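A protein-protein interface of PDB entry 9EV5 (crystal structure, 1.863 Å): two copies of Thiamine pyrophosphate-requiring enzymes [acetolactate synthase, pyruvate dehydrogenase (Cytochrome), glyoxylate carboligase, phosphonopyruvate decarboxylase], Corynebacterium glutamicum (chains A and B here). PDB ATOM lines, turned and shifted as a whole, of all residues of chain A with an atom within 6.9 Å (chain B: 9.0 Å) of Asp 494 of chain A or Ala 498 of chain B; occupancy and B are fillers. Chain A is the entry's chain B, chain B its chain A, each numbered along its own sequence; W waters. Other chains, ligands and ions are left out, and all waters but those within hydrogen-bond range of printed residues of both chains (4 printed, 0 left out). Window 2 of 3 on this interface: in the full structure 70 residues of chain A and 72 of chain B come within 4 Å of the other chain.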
ATOM      1  N   VAL A 490     -35.134 -15.042   6.122  1.00  0.00           N
ATOM      2  CA  VAL A 490     -33.866 -14.537   6.598  1.00  0.00           C
ATOM      3  C   VAL A 490     -33.939 -13.018   6.665  1.00  0.00           C
ATOM      4  O   VAL A 490     -34.437 -12.380   5.740  1.00  0.00           O
ATOM      5  CB  VAL A 490     -32.729 -14.971   5.673  1.00  0.00           C
ATOM      6  CG1 VAL A 490     -31.401 -14.363   6.125  1.00  0.00           C
ATOM      7  CG2 VAL A 490     -32.659 -16.485   5.579  1.00  0.00           C
ATOM      8  N   ASN A 491     -33.443 -12.425   7.762  1.00  0.00           N
ATOM      9  CA  ASN A 491     -33.456 -10.977   7.915  1.00  0.00           C
ATOM     10  C   ASN A 491     -32.105 -10.412   7.473  1.00  0.00           C
ATOM     11  O   ASN A 491     -31.165 -10.370   8.264  1.00  0.00           O
ATOM     12  CB  ASN A 491     -33.752 -10.597   9.367  1.00  0.00           C
ATOM     13  CG  ASN A 491     -34.102  -9.146   9.513  1.00  0.00           C
ATOM     14  OD1 ASN A 491     -33.478  -8.258   8.890  1.00  0.00           O
ATOM     15  ND2 ASN A 491     -35.110  -8.866  10.345  1.00  0.00           N
ATOM     16  N   PHE A 492     -32.013  -9.970   6.223  1.00  0.00           N
ATOM     17  CA  PHE A 492     -30.767  -9.425   5.690  1.00  0.00           C
ATOM     18  C   PHE A 492     -30.448  -8.041   6.226  1.00  0.00           C
ATOM     19  O   PHE A 492     -29.281  -7.696   6.299  1.00  0.00           O
ATOM     20  CB  PHE A 492     -30.756  -9.450   4.167  1.00  0.00           C
ATOM     21  CG  PHE A 492     -30.693 -10.847   3.606  1.00  0.00           C
ATOM     22  CD1 PHE A 492     -29.500 -11.557   3.598  1.00  0.00           C
ATOM     23  CD2 PHE A 492     -31.826 -11.459   3.097  1.00  0.00           C
ATOM     24  CE1 PHE A 492     -29.436 -12.847   3.064  1.00  0.00           C
ATOM     25  CE2 PHE A 492     -31.763 -12.755   2.566  1.00  0.00           C
ATOM     26  CZ  PHE A 492     -30.563 -13.432   2.537  1.00  0.00           C
ATOM     27  N   ALA A 493     -31.469  -7.261   6.667  1.00  0.00           N
ATOM     28  CA  ALA A 493     -31.216  -5.949   7.256  1.00  0.00           C
ATOM     29  C   ALA A 493     -30.450  -6.133   8.580  1.00  0.00           C
ATOM     30  O   ALA A 493     -29.516  -5.390   8.846  1.00  0.00           O
ATOM     31  CB  ALA A 493     -32.535  -5.215   7.506  1.00  0.00           C
ATOM     32  N   ASP A 494     -30.852  -7.108   9.405  1.00  0.00           N
ATOM     33  CA  ASP A 494     -30.180  -7.376  10.656  1.00  0.00           C
ATOM     34  C   ASP A 494     -28.758  -7.892  10.427  1.00  0.00           C
ATOM     35  O   ASP A 494     -27.842  -7.480  11.152  1.00  0.00           O
ATOM     36  CB  ASP A 494     -30.977  -8.375  11.497  1.00  0.00           C
ATOM     37  CG  ASP A 494     -32.237  -7.817  12.130  1.00  0.00           C
ATOM     38  OD1 ASP A 494     -32.459  -6.582  12.044  1.00  0.00           O
ATOM     39  OD2 ASP A 494     -33.010  -8.608  12.689  1.00  0.00           O
ATOM     40  N   ILE A 495     -28.561  -8.783   9.427  1.00  0.00           N
ATOM     41  CA  ILE A 495     -27.232  -9.282   9.099  1.00  0.00           C
ATOM     42  C   ILE A 495     -26.337  -8.130   8.612  1.00  0.00           C
ATOM     43  O   ILE A 495     -25.199  -8.013   9.058  1.00  0.00           O
ATOM     44  CB  ILE A 495     -27.311 -10.442   8.085  1.00  0.00           C
ATOM     45  CG1 ILE A 495     -28.070 -11.638   8.691  1.00  0.00           C
ATOM     46  CG2 ILE A 495     -25.923 -10.869   7.618  1.00  0.00           C
ATOM     47  CD1 ILE A 495     -28.369 -12.798   7.722  1.00  0.00           C
ATOM     48  N   ALA A 496     -26.860  -7.250   7.748  1.00  0.00           N
ATOM     49  CA  ALA A 496     -26.109  -6.097   7.261  1.00  0.00           C
ATOM     50  C   ALA A 496     -25.752  -5.171   8.416  1.00  0.00           C
ATOM     51  O   ALA A 496     -24.601  -4.743   8.497  1.00  0.00           O
ATOM     52  CB  ALA A 496     -26.884  -5.339   6.196  1.00  0.00           C
ATOM     53  N   ALA A 497     -26.701  -4.899   9.325  1.00  0.00           N
ATOM     54  CA  ALA A 497     -26.433  -4.063  10.488  1.00  0.00           C
ATOM     55  C   ALA A 497     -25.361  -4.711  11.392  1.00  0.00           C
ATOM     56  O   ALA A 497     -24.433  -4.027  11.804  1.00  0.00           O
ATOM     57  CB  ALA A 497     -27.723  -3.801  11.270  1.00  0.00           C
ATOM     58  N   ALA A 498     -25.406  -6.050  11.588  1.00  0.00           N
ATOM     59  CA  ALA A 498     -24.394  -6.744  12.404  1.00  0.00           C
ATOM     60  C   ALA A 498     -22.984  -6.653  11.758  1.00  0.00           C
ATOM     61  O   ALA A 498     -21.978  -6.684  12.462  1.00  0.00           O
ATOM     62  CB  ALA A 498     -24.788  -8.199  12.611  1.00  0.00           C
ATOM     63  N   ALA A 499     -22.929  -6.517  10.422  1.00  0.00           N
ATOM     64  CA  ALA A 499     -21.668  -6.357   9.712  1.00  0.00           C
ATOM     65  C   ALA A 499     -21.193  -4.883   9.640  1.00  0.00           C
ATOM     66  O   ALA A 499     -20.191  -4.626   9.003  1.00  0.00           O
ATOM     67  CB  ALA A 499     -21.787  -6.928   8.313  1.00  0.00           C
ATOM     68  N   ILE A 501     -23.138  -2.279   8.350  1.00  0.00           N
ATOM     69  CA  ILE A 501     -23.712  -1.590   7.205  1.00  0.00           C
ATOM     70  C   ILE A 501     -25.079  -1.009   7.553  1.00  0.00           C
ATOM     71  O   ILE A 501     -25.911  -1.708   8.124  1.00  0.00           O
ATOM     72  CB  ILE A 501     -23.793  -2.542   5.973  1.00  0.00           C
ATOM     73  CG1 ILE A 501     -22.373  -3.066   5.598  1.00  0.00           C
ATOM     74  CG2 ILE A 501     -24.467  -1.848   4.783  1.00  0.00           C
ATOM     75  CD1 ILE A 501     -22.356  -4.088   4.588  1.00  0.00           C
ATOM     76  N   SER A 503     -28.809  -0.266   7.310  1.00  0.00           N
ATOM     77  CA  SER A 503     -29.809  -1.120   6.674  1.00  0.00           C
ATOM     78  C   SER A 503     -31.235  -0.710   6.965  1.00  0.00           C
ATOM     79  O   SER A 503     -31.525  -0.084   7.980  1.00  0.00           O
ATOM     80  CB  SER A 503     -29.578  -2.583   7.036  1.00  0.00           C
ATOM     81  OG  SER A 503     -29.898  -2.818   8.397  1.00  0.00           O
ATOM     82  N   ARG A 505     -35.349  -2.363   6.509  1.00  0.00           N
ATOM     83  CA  ARG A 505     -36.165  -3.523   6.180  1.00  0.00           C
ATOM     84  C   ARG A 505     -37.541  -2.973   5.763  1.00  0.00           C
ATOM     85  O   ARG A 505     -38.148  -2.220   6.517  1.00  0.00           O
ATOM     86  CB  ARG A 505     -36.267  -4.507   7.355  1.00  0.00           C
ATOM     87  CG  ARG A 505     -36.977  -5.798   6.933  1.00  0.00           C
ATOM     88  CD  ARG A 505     -36.490  -6.982   7.733  1.00  0.00           C
ATOM     89  NE  ARG A 505     -37.414  -8.118   7.704  1.00  0.00           N
ATOM     90  CZ  ARG A 505     -37.196  -9.248   7.038  1.00  0.00           C
ATOM     91  NH1 ARG A 505     -36.123  -9.380   6.271  1.00  0.00           N
ATOM     92  NH2 ARG A 505     -38.057 -10.248   7.119  1.00  0.00           N
ATOM     93  N   LEU A 527     -27.937  -1.547   2.770  1.00  0.00           N
ATOM     94  CA  LEU A 527     -28.620  -2.740   2.329  1.00  0.00           C
ATOM     95  C   LEU A 527     -30.114  -2.496   2.578  1.00  0.00           C
ATOM     96  O   LEU A 527     -30.516  -2.208   3.697  1.00  0.00           O
ATOM     97  CB  LEU A 527     -28.148  -4.001   3.054  1.00  0.00           C
ATOM     98  CG  LEU A 527     -28.779  -5.291   2.532  1.00  0.00           C
ATOM     99  CD1 LEU A 527     -27.761  -6.355   2.339  1.00  0.00           C
ATOM    100  CD2 LEU A 527     -29.936  -5.755   3.420  1.00  0.00           C
ATOM    101  N   ASP A 529     -33.467  -4.361   2.650  1.00  0.00           N
ATOM    102  CA  ASP A 529     -34.034  -5.702   2.648  1.00  0.00           C
ATOM    103  C   ASP A 529     -35.544  -5.603   2.404  1.00  0.00           C
ATOM    104  O   ASP A 529     -36.280  -5.218   3.302  1.00  0.00           O
ATOM    105  CB  ASP A 529     -33.705  -6.377   3.975  1.00  0.00           C
ATOM    106  CG  ASP A 529     -34.213  -7.793   4.139  1.00  0.00           C
ATOM    107  OD1 ASP A 529     -34.771  -8.338   3.178  1.00  0.00           O
ATOM    108  OD2 ASP A 529     -34.095  -8.339   5.250  1.00  0.00           O
ATOM    109  N   LEU B 448     -24.087 -20.085   7.437  1.00  0.00           N
ATOM    110  CA  LEU B 448     -24.743 -19.900   8.742  1.00  0.00           C
ATOM    111  C   LEU B 448     -26.287 -20.052   8.536  1.00  0.00           C
ATOM    112  O   LEU B 448     -26.994 -20.541   9.420  1.00  0.00           O
ATOM    113  CB  LEU B 448     -24.415 -18.519   9.363  1.00  0.00           C
ATOM    114  CG  LEU B 448     -22.954 -18.320   9.891  1.00  0.00           C
ATOM    115  CD1 LEU B 448     -22.771 -16.917  10.488  1.00  0.00           C
ATOM    116  CD2 LEU B 448     -22.604 -19.377  10.952  1.00  0.00           C
ATOM    117  N   LEU B 449     -26.802 -19.653   7.360  1.00  0.00           N
ATOM    118  CA  LEU B 449     -28.229 -19.789   7.039  1.00  0.00           C
ATOM    119  C   LEU B 449     -28.656 -21.268   6.918  1.00  0.00           C
ATOM    120  O   LEU B 449     -29.755 -21.626   7.336  1.00  0.00           O
ATOM    121  CB  LEU B 449     -28.566 -19.019   5.762  1.00  0.00           C
ATOM    122  CG  LEU B 449     -28.143 -17.534   5.743  1.00  0.00           C
ATOM    123  CD1 LEU B 449     -28.569 -16.868   4.426  1.00  0.00           C
ATOM    124  CD2 LEU B 449     -28.687 -16.752   6.940  1.00  0.00           C
ATOM    125  N   LYS B 452     -28.928 -22.848  10.429  1.00  0.00           N
ATOM    126  CA  LYS B 452     -30.179 -22.407  11.027  1.00  0.00           C
ATOM    127  C   LYS B 452     -31.364 -23.161  10.419  1.00  0.00           C
ATOM    128  O   LYS B 452     -32.188 -23.716  11.151  1.00  0.00           O
ATOM    129  CB  LYS B 452     -30.340 -20.879  10.865  1.00  0.00           C
ATOM    130  CG  LYS B 452     -31.736 -20.308  11.246  1.00  0.00           C
ATOM    131  CD  LYS B 452     -32.024 -20.440  12.723  1.00  0.00           C
ATOM    132  CE  LYS B 452     -33.347 -19.814  13.123  1.00  0.00           C
ATOM    133  NZ  LYS B 452     -34.525 -20.619  12.654  1.00  0.00           N
ATOM    134  N   ASN B 491     -17.733  -8.750  13.904  1.00  0.00           N
ATOM    135  CA  ASN B 491     -18.415  -9.358  15.047  1.00  0.00           C
ATOM    136  C   ASN B 491     -19.253 -10.509  14.551  1.00  0.00           C
ATOM    137  O   ASN B 491     -20.381 -10.310  14.122  1.00  0.00           O
ATOM    138  CB  ASN B 491     -19.256  -8.333  15.787  1.00  0.00           C
ATOM    139  CG  ASN B 491     -19.723  -8.817  17.133  1.00  0.00           C
ATOM    140  OD1 ASN B 491     -20.142  -9.977  17.306  1.00  0.00           O
ATOM    141  ND2 ASN B 491     -19.675  -7.933  18.106  1.00  0.00           N
ATOM    142  N   PHE B 492     -18.699 -11.713  14.595  1.00  0.00           N
ATOM    143  CA  PHE B 492     -19.401 -12.903  14.116  1.00  0.00           C
ATOM    144  C   PHE B 492     -20.532 -13.323  15.050  1.00  0.00           C
ATOM    145  O   PHE B 492     -21.486 -13.923  14.584  1.00  0.00           O
ATOM    146  CB  PHE B 492     -18.441 -14.055  13.873  1.00  0.00           C
ATOM    147  CG  PHE B 492     -17.549 -13.803  12.681  1.00  0.00           C
ATOM    148  CD1 PHE B 492     -18.042 -13.926  11.386  1.00  0.00           C
ATOM    149  CD2 PHE B 492     -16.230 -13.402  12.854  1.00  0.00           C
ATOM    150  CE1 PHE B 492     -17.227 -13.675  10.291  1.00  0.00           C
ATOM    151  CE2 PHE B 492     -15.418 -13.156  11.750  1.00  0.00           C
ATOM    152  CZ  PHE B 492     -15.922 -13.290  10.479  1.00  0.00           C
ATOM    153  N   ALA B 493     -20.454 -12.995  16.353  1.00  0.00           N
ATOM    154  CA  ALA B 493     -21.536 -13.307  17.285  1.00  0.00           C
ATOM    155  C   ALA B 493     -22.790 -12.532  16.886  1.00  0.00           C
ATOM    156  O   ALA B 493     -23.890 -13.087  16.905  1.00  0.00           O
ATOM    157  CB  ALA B 493     -21.133 -12.951  18.724  1.00  0.00           C
ATOM    158  N   ASP B 494     -22.633 -11.254  16.510  1.00  0.00           N
ATOM    159  CA  ASP B 494     -23.778 -10.437  16.097  1.00  0.00           C
ATOM    160  C   ASP B 494     -24.340 -10.936  14.800  1.00  0.00           C
ATOM    161  O   ASP B 494     -25.558 -10.974  14.657  1.00  0.00           O
ATOM    162  CB  ASP B 494     -23.405  -8.957  15.993  1.00  0.00           C
ATOM    163  CG  ASP B 494     -23.135  -8.281  17.313  1.00  0.00           C
ATOM    164  OD1 ASP B 494     -23.382  -8.919  18.376  1.00  0.00           O
ATOM    165  OD2 ASP B 494     -22.666  -7.114  17.295  1.00  0.00           O
ATOM    166  N   ILE B 495     -23.470 -11.317  13.845  1.00  0.00           N
ATOM    167  CA  ILE B 495     -23.914 -11.856  12.565  1.00  0.00           C
ATOM    168  C   ILE B 495     -24.675 -13.165  12.775  1.00  0.00           C
ATOM    169  O   ILE B 495     -25.763 -13.302  12.248  1.00  0.00           O
ATOM    170  CB  ILE B 495     -22.735 -11.986  11.567  1.00  0.00           C
ATOM    171  CG1 ILE B 495     -22.187 -10.592  11.199  1.00  0.00           C
ATOM    172  CG2 ILE B 495     -23.147 -12.725  10.328  1.00  0.00           C
ATOM    173  CD1 ILE B 495     -20.870 -10.615  10.324  1.00  0.00           C
ATOM    174  N   ALA B 496     -24.148 -14.080  13.591  1.00  0.00           N
ATOM    175  CA  ALA B 496     -24.818 -15.335  13.899  1.00  0.00           C
ATOM    176  C   ALA B 496     -26.135 -15.102  14.583  1.00  0.00           C
ATOM    177  O   ALA B 496     -27.122 -15.723  14.191  1.00  0.00           O
ATOM    178  CB  ALA B 496     -23.942 -16.207  14.758  1.00  0.00           C
ATOM    179  N   ALA B 497     -26.202 -14.142  15.541  1.00  0.00           N
ATOM    180  CA  ALA B 497     -27.470 -13.805  16.190  1.00  0.00           C
ATOM    181  C   ALA B 497     -28.461 -13.217  15.187  1.00  0.00           C
ATOM    182  O   ALA B 497     -29.636 -13.580  15.219  1.00  0.00           O
ATOM    183  CB  ALA B 497     -27.235 -12.840  17.336  1.00  0.00           C
ATOM    184  N   ALA B 498     -28.002 -12.374  14.256  1.00  0.00           N
ATOM    185  CA  ALA B 498     -28.888 -11.811  13.219  1.00  0.00           C
ATOM    186  C   ALA B 498     -29.433 -12.886  12.277  1.00  0.00           C
ATOM    187  O   ALA B 498     -30.509 -12.711  11.703  1.00  0.00           O
ATOM    188  CB  ALA B 498     -28.167 -10.737  12.417  1.00  0.00           C
ATOM    189  N   ALA B 499     -28.705 -14.007  12.133  1.00  0.00           N
ATOM    190  CA  ALA B 499     -29.153 -15.146  11.351  1.00  0.00           C
ATOM    191  C   ALA B 499     -30.024 -16.141  12.158  1.00  0.00           C
ATOM    192  O   ALA B 499     -30.345 -17.202  11.636  1.00  0.00           O
ATOM    193  CB  ALA B 499     -27.949 -15.874  10.760  1.00  0.00           C
ATOM    194  N   GLY B 500     -30.325 -15.837  13.417  1.00  0.00           N
ATOM    195  CA  GLY B 500     -31.168 -16.675  14.259  1.00  0.00           C
ATOM    196  C   GLY B 500     -30.438 -17.753  15.030  1.00  0.00           C
ATOM    197  O   GLY B 500     -31.063 -18.696  15.527  1.00  0.00           O
ATOM    198  N   ILE B 501     -29.113 -17.614  15.161  1.00  0.00           N
ATOM    199  CA  ILE B 501     -28.316 -18.625  15.842  1.00  0.00           C
ATOM    200  C   ILE B 501     -27.850 -18.091  17.160  1.00  0.00           C
ATOM    201  O   ILE B 501     -27.290 -16.992  17.186  1.00  0.00           O
ATOM    202  CB  ILE B 501     -27.101 -19.061  14.973  1.00  0.00           C
ATOM    203  CG1 ILE B 501     -27.574 -19.693  13.639  1.00  0.00           C
ATOM    204  CG2 ILE B 501     -26.172 -20.015  15.756  1.00  0.00           C
ATOM    205  CD1 ILE B 501     -26.521 -19.893  12.687  1.00  0.00           C
ATOM    206  N   LYS B 502     -28.014 -18.880  18.259  1.00  0.00           N
ATOM    207  CA  LYS B 502     -27.501 -18.534  19.592  1.00  0.00           C
ATOM    208  C   LYS B 502     -25.993 -18.252  19.492  1.00  0.00           C
ATOM    209  O   LYS B 502     -25.269 -19.021  18.842  1.00  0.00           O
ATOM    210  CB  LYS B 502     -27.746 -19.702  20.564  1.00  0.00           C
ATOM    211  CG  LYS B 502     -27.144 -19.534  21.955  1.00  0.00           C
ATOM    212  CD  LYS B 502     -27.887 -18.543  22.772  1.00  0.00           C
ATOM    213  CE  LYS B 502     -27.476 -18.591  24.229  1.00  0.00           C
ATOM    214  NZ  LYS B 502     -28.470 -17.864  25.052  1.00  0.00           N
ATOM    215  N   SER B 503     -25.550 -17.103  19.999  1.00  0.00           N
ATOM    216  CA  SER B 503     -24.140 -16.759  19.906  1.00  0.00           C
ATOM    217  C   SER B 503     -23.555 -16.180  21.183  1.00  0.00           C
ATOM    218  O   SER B 503     -24.263 -15.623  22.018  1.00  0.00           O
ATOM    219  CB  SER B 503     -23.888 -15.837  18.729  1.00  0.00           C
ATOM    220  OG  SER B 503     -24.435 -14.563  18.995  1.00  0.00           O
HETATM  221  O   HOH W   1     -22.026  -5.680  15.042  1.00  0.00           O
HETATM  222  O   HOH W   2     -19.234  -6.873  12.401  1.00  0.00           O
HETATM  223  O   HOH W   3     -32.871 -11.457  13.005  1.00  0.00           O
HETATM  224  O   HOH W   4     -32.294 -13.894   9.888  1.00  0.00           O
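Water W1 lies within hydrogen-bond range of OD2 of Asp 494 of chain B and O of Ala 498 of chain A.
Water W2 bridges O of Ala 498 of chain A (2.8 Å) and N of Asn 491 of chain B (2.8 Å).
Water W4 bridges O of Ala 498 of chain B (2.8 Å) and N of Asn 491 of chain A (2.8 Å).
Water W3 bridges OD2 of Asp 494 of chain A (2.9 Å) and O of Ala 498 of chain B (3.0 Å).
Asp 494 of chain A touches Ala 498 of chain B, and with the chains exchanged Ala 498 of chain A touches Asp 494 of chain B.
Ile 495 of chain A touches Ala 498 of chain B, and with the chains exchanged Ala 498 of chain A touches Ile 495 of chain B.
Of the 5 pairs that touch across the chains among the printed residues, 4 have their exchanged pair printed and touching as well.
CD2 of Leu 449 of chain B touches CG1 of Val 490 of chain A, 3.7 Å away.
Asp 494 of chain A touches Ala 498 of chain B.
CB of Ala 498 of chain B touches N of Ile 495 of chain A, 3.6 Å away.
Asp 494 of chain B touches Ala 498 of chain A (O to CB, 3.5 Å).
N of Ile 495 of chain B touches CB of Ala 498 of chain A, at 3.6 Å.
Printed residues of chain B that touch a printed residue of chain A: Leu 449, Asp 494, Ile 495 and Ala 498.
Hydrophobic or aromatic side chains of chain B that line the printed part of chain A: Leu 449, Ile 495 and Ala 498.
Along chain B the printed residues that touch a printed residue of chain A span positions 449 to 498.
Among the printed residues, no Asp or Glu carboxylate lies within 4 Å of a Lys or Arg side-chain nitrogen of the other chain.
Asn 491 of chain A touches none of the printed residues of chain B.
No residue of chain B comes within 4 Å of Ala 493 of chain A.
Of the printed residues of chain B, Asp 494 of chain A touches Ala 498 (3.5 Å).
Of the printed residues of chain B, Ile 495 of chain A touches Ala 498 (3.6 Å).
Of the printed residues of chain B, Ala 498 of chain A touches Asp 494 and Ile 495.
Of the printed residues of chain A, Asp 494 of chain B touches Ala 498.
Of the printed residues of chain A, Ile 495 of chain B touches Ala 498 (3.6 Å).
Of chain A, only Asp 494 and Ile 495 come within 4 Å of Ala 498 of chain B.
Ile 501 of chain B touches none of the printed residues of chain A.
The nearest residue of chain B that does not touch Asp 494 of chain A is Asp 494 of chain B (5.5 Å).
The nearest printed residue of chain A that does not touch Leu 449 of chain B is Ile 495 of chain A (4.04 Å).
OD1 of Asn 491 of chain B sits at hydrogen-bond distance from N of Asp 494 of chain B (2.9 Å).
The guanidinium group (NH1) of Arg 505 of chain A is in hydrogen-bond range of the backbone carbonyl oxygen (O) of Val 490 of chain A, 3.5 Å away.
The side-chain amide oxygen of Asn 491 of chain A lies within hydrogen-bond range of the backbone NH of Asp 494 of chain A (2.9 Å).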
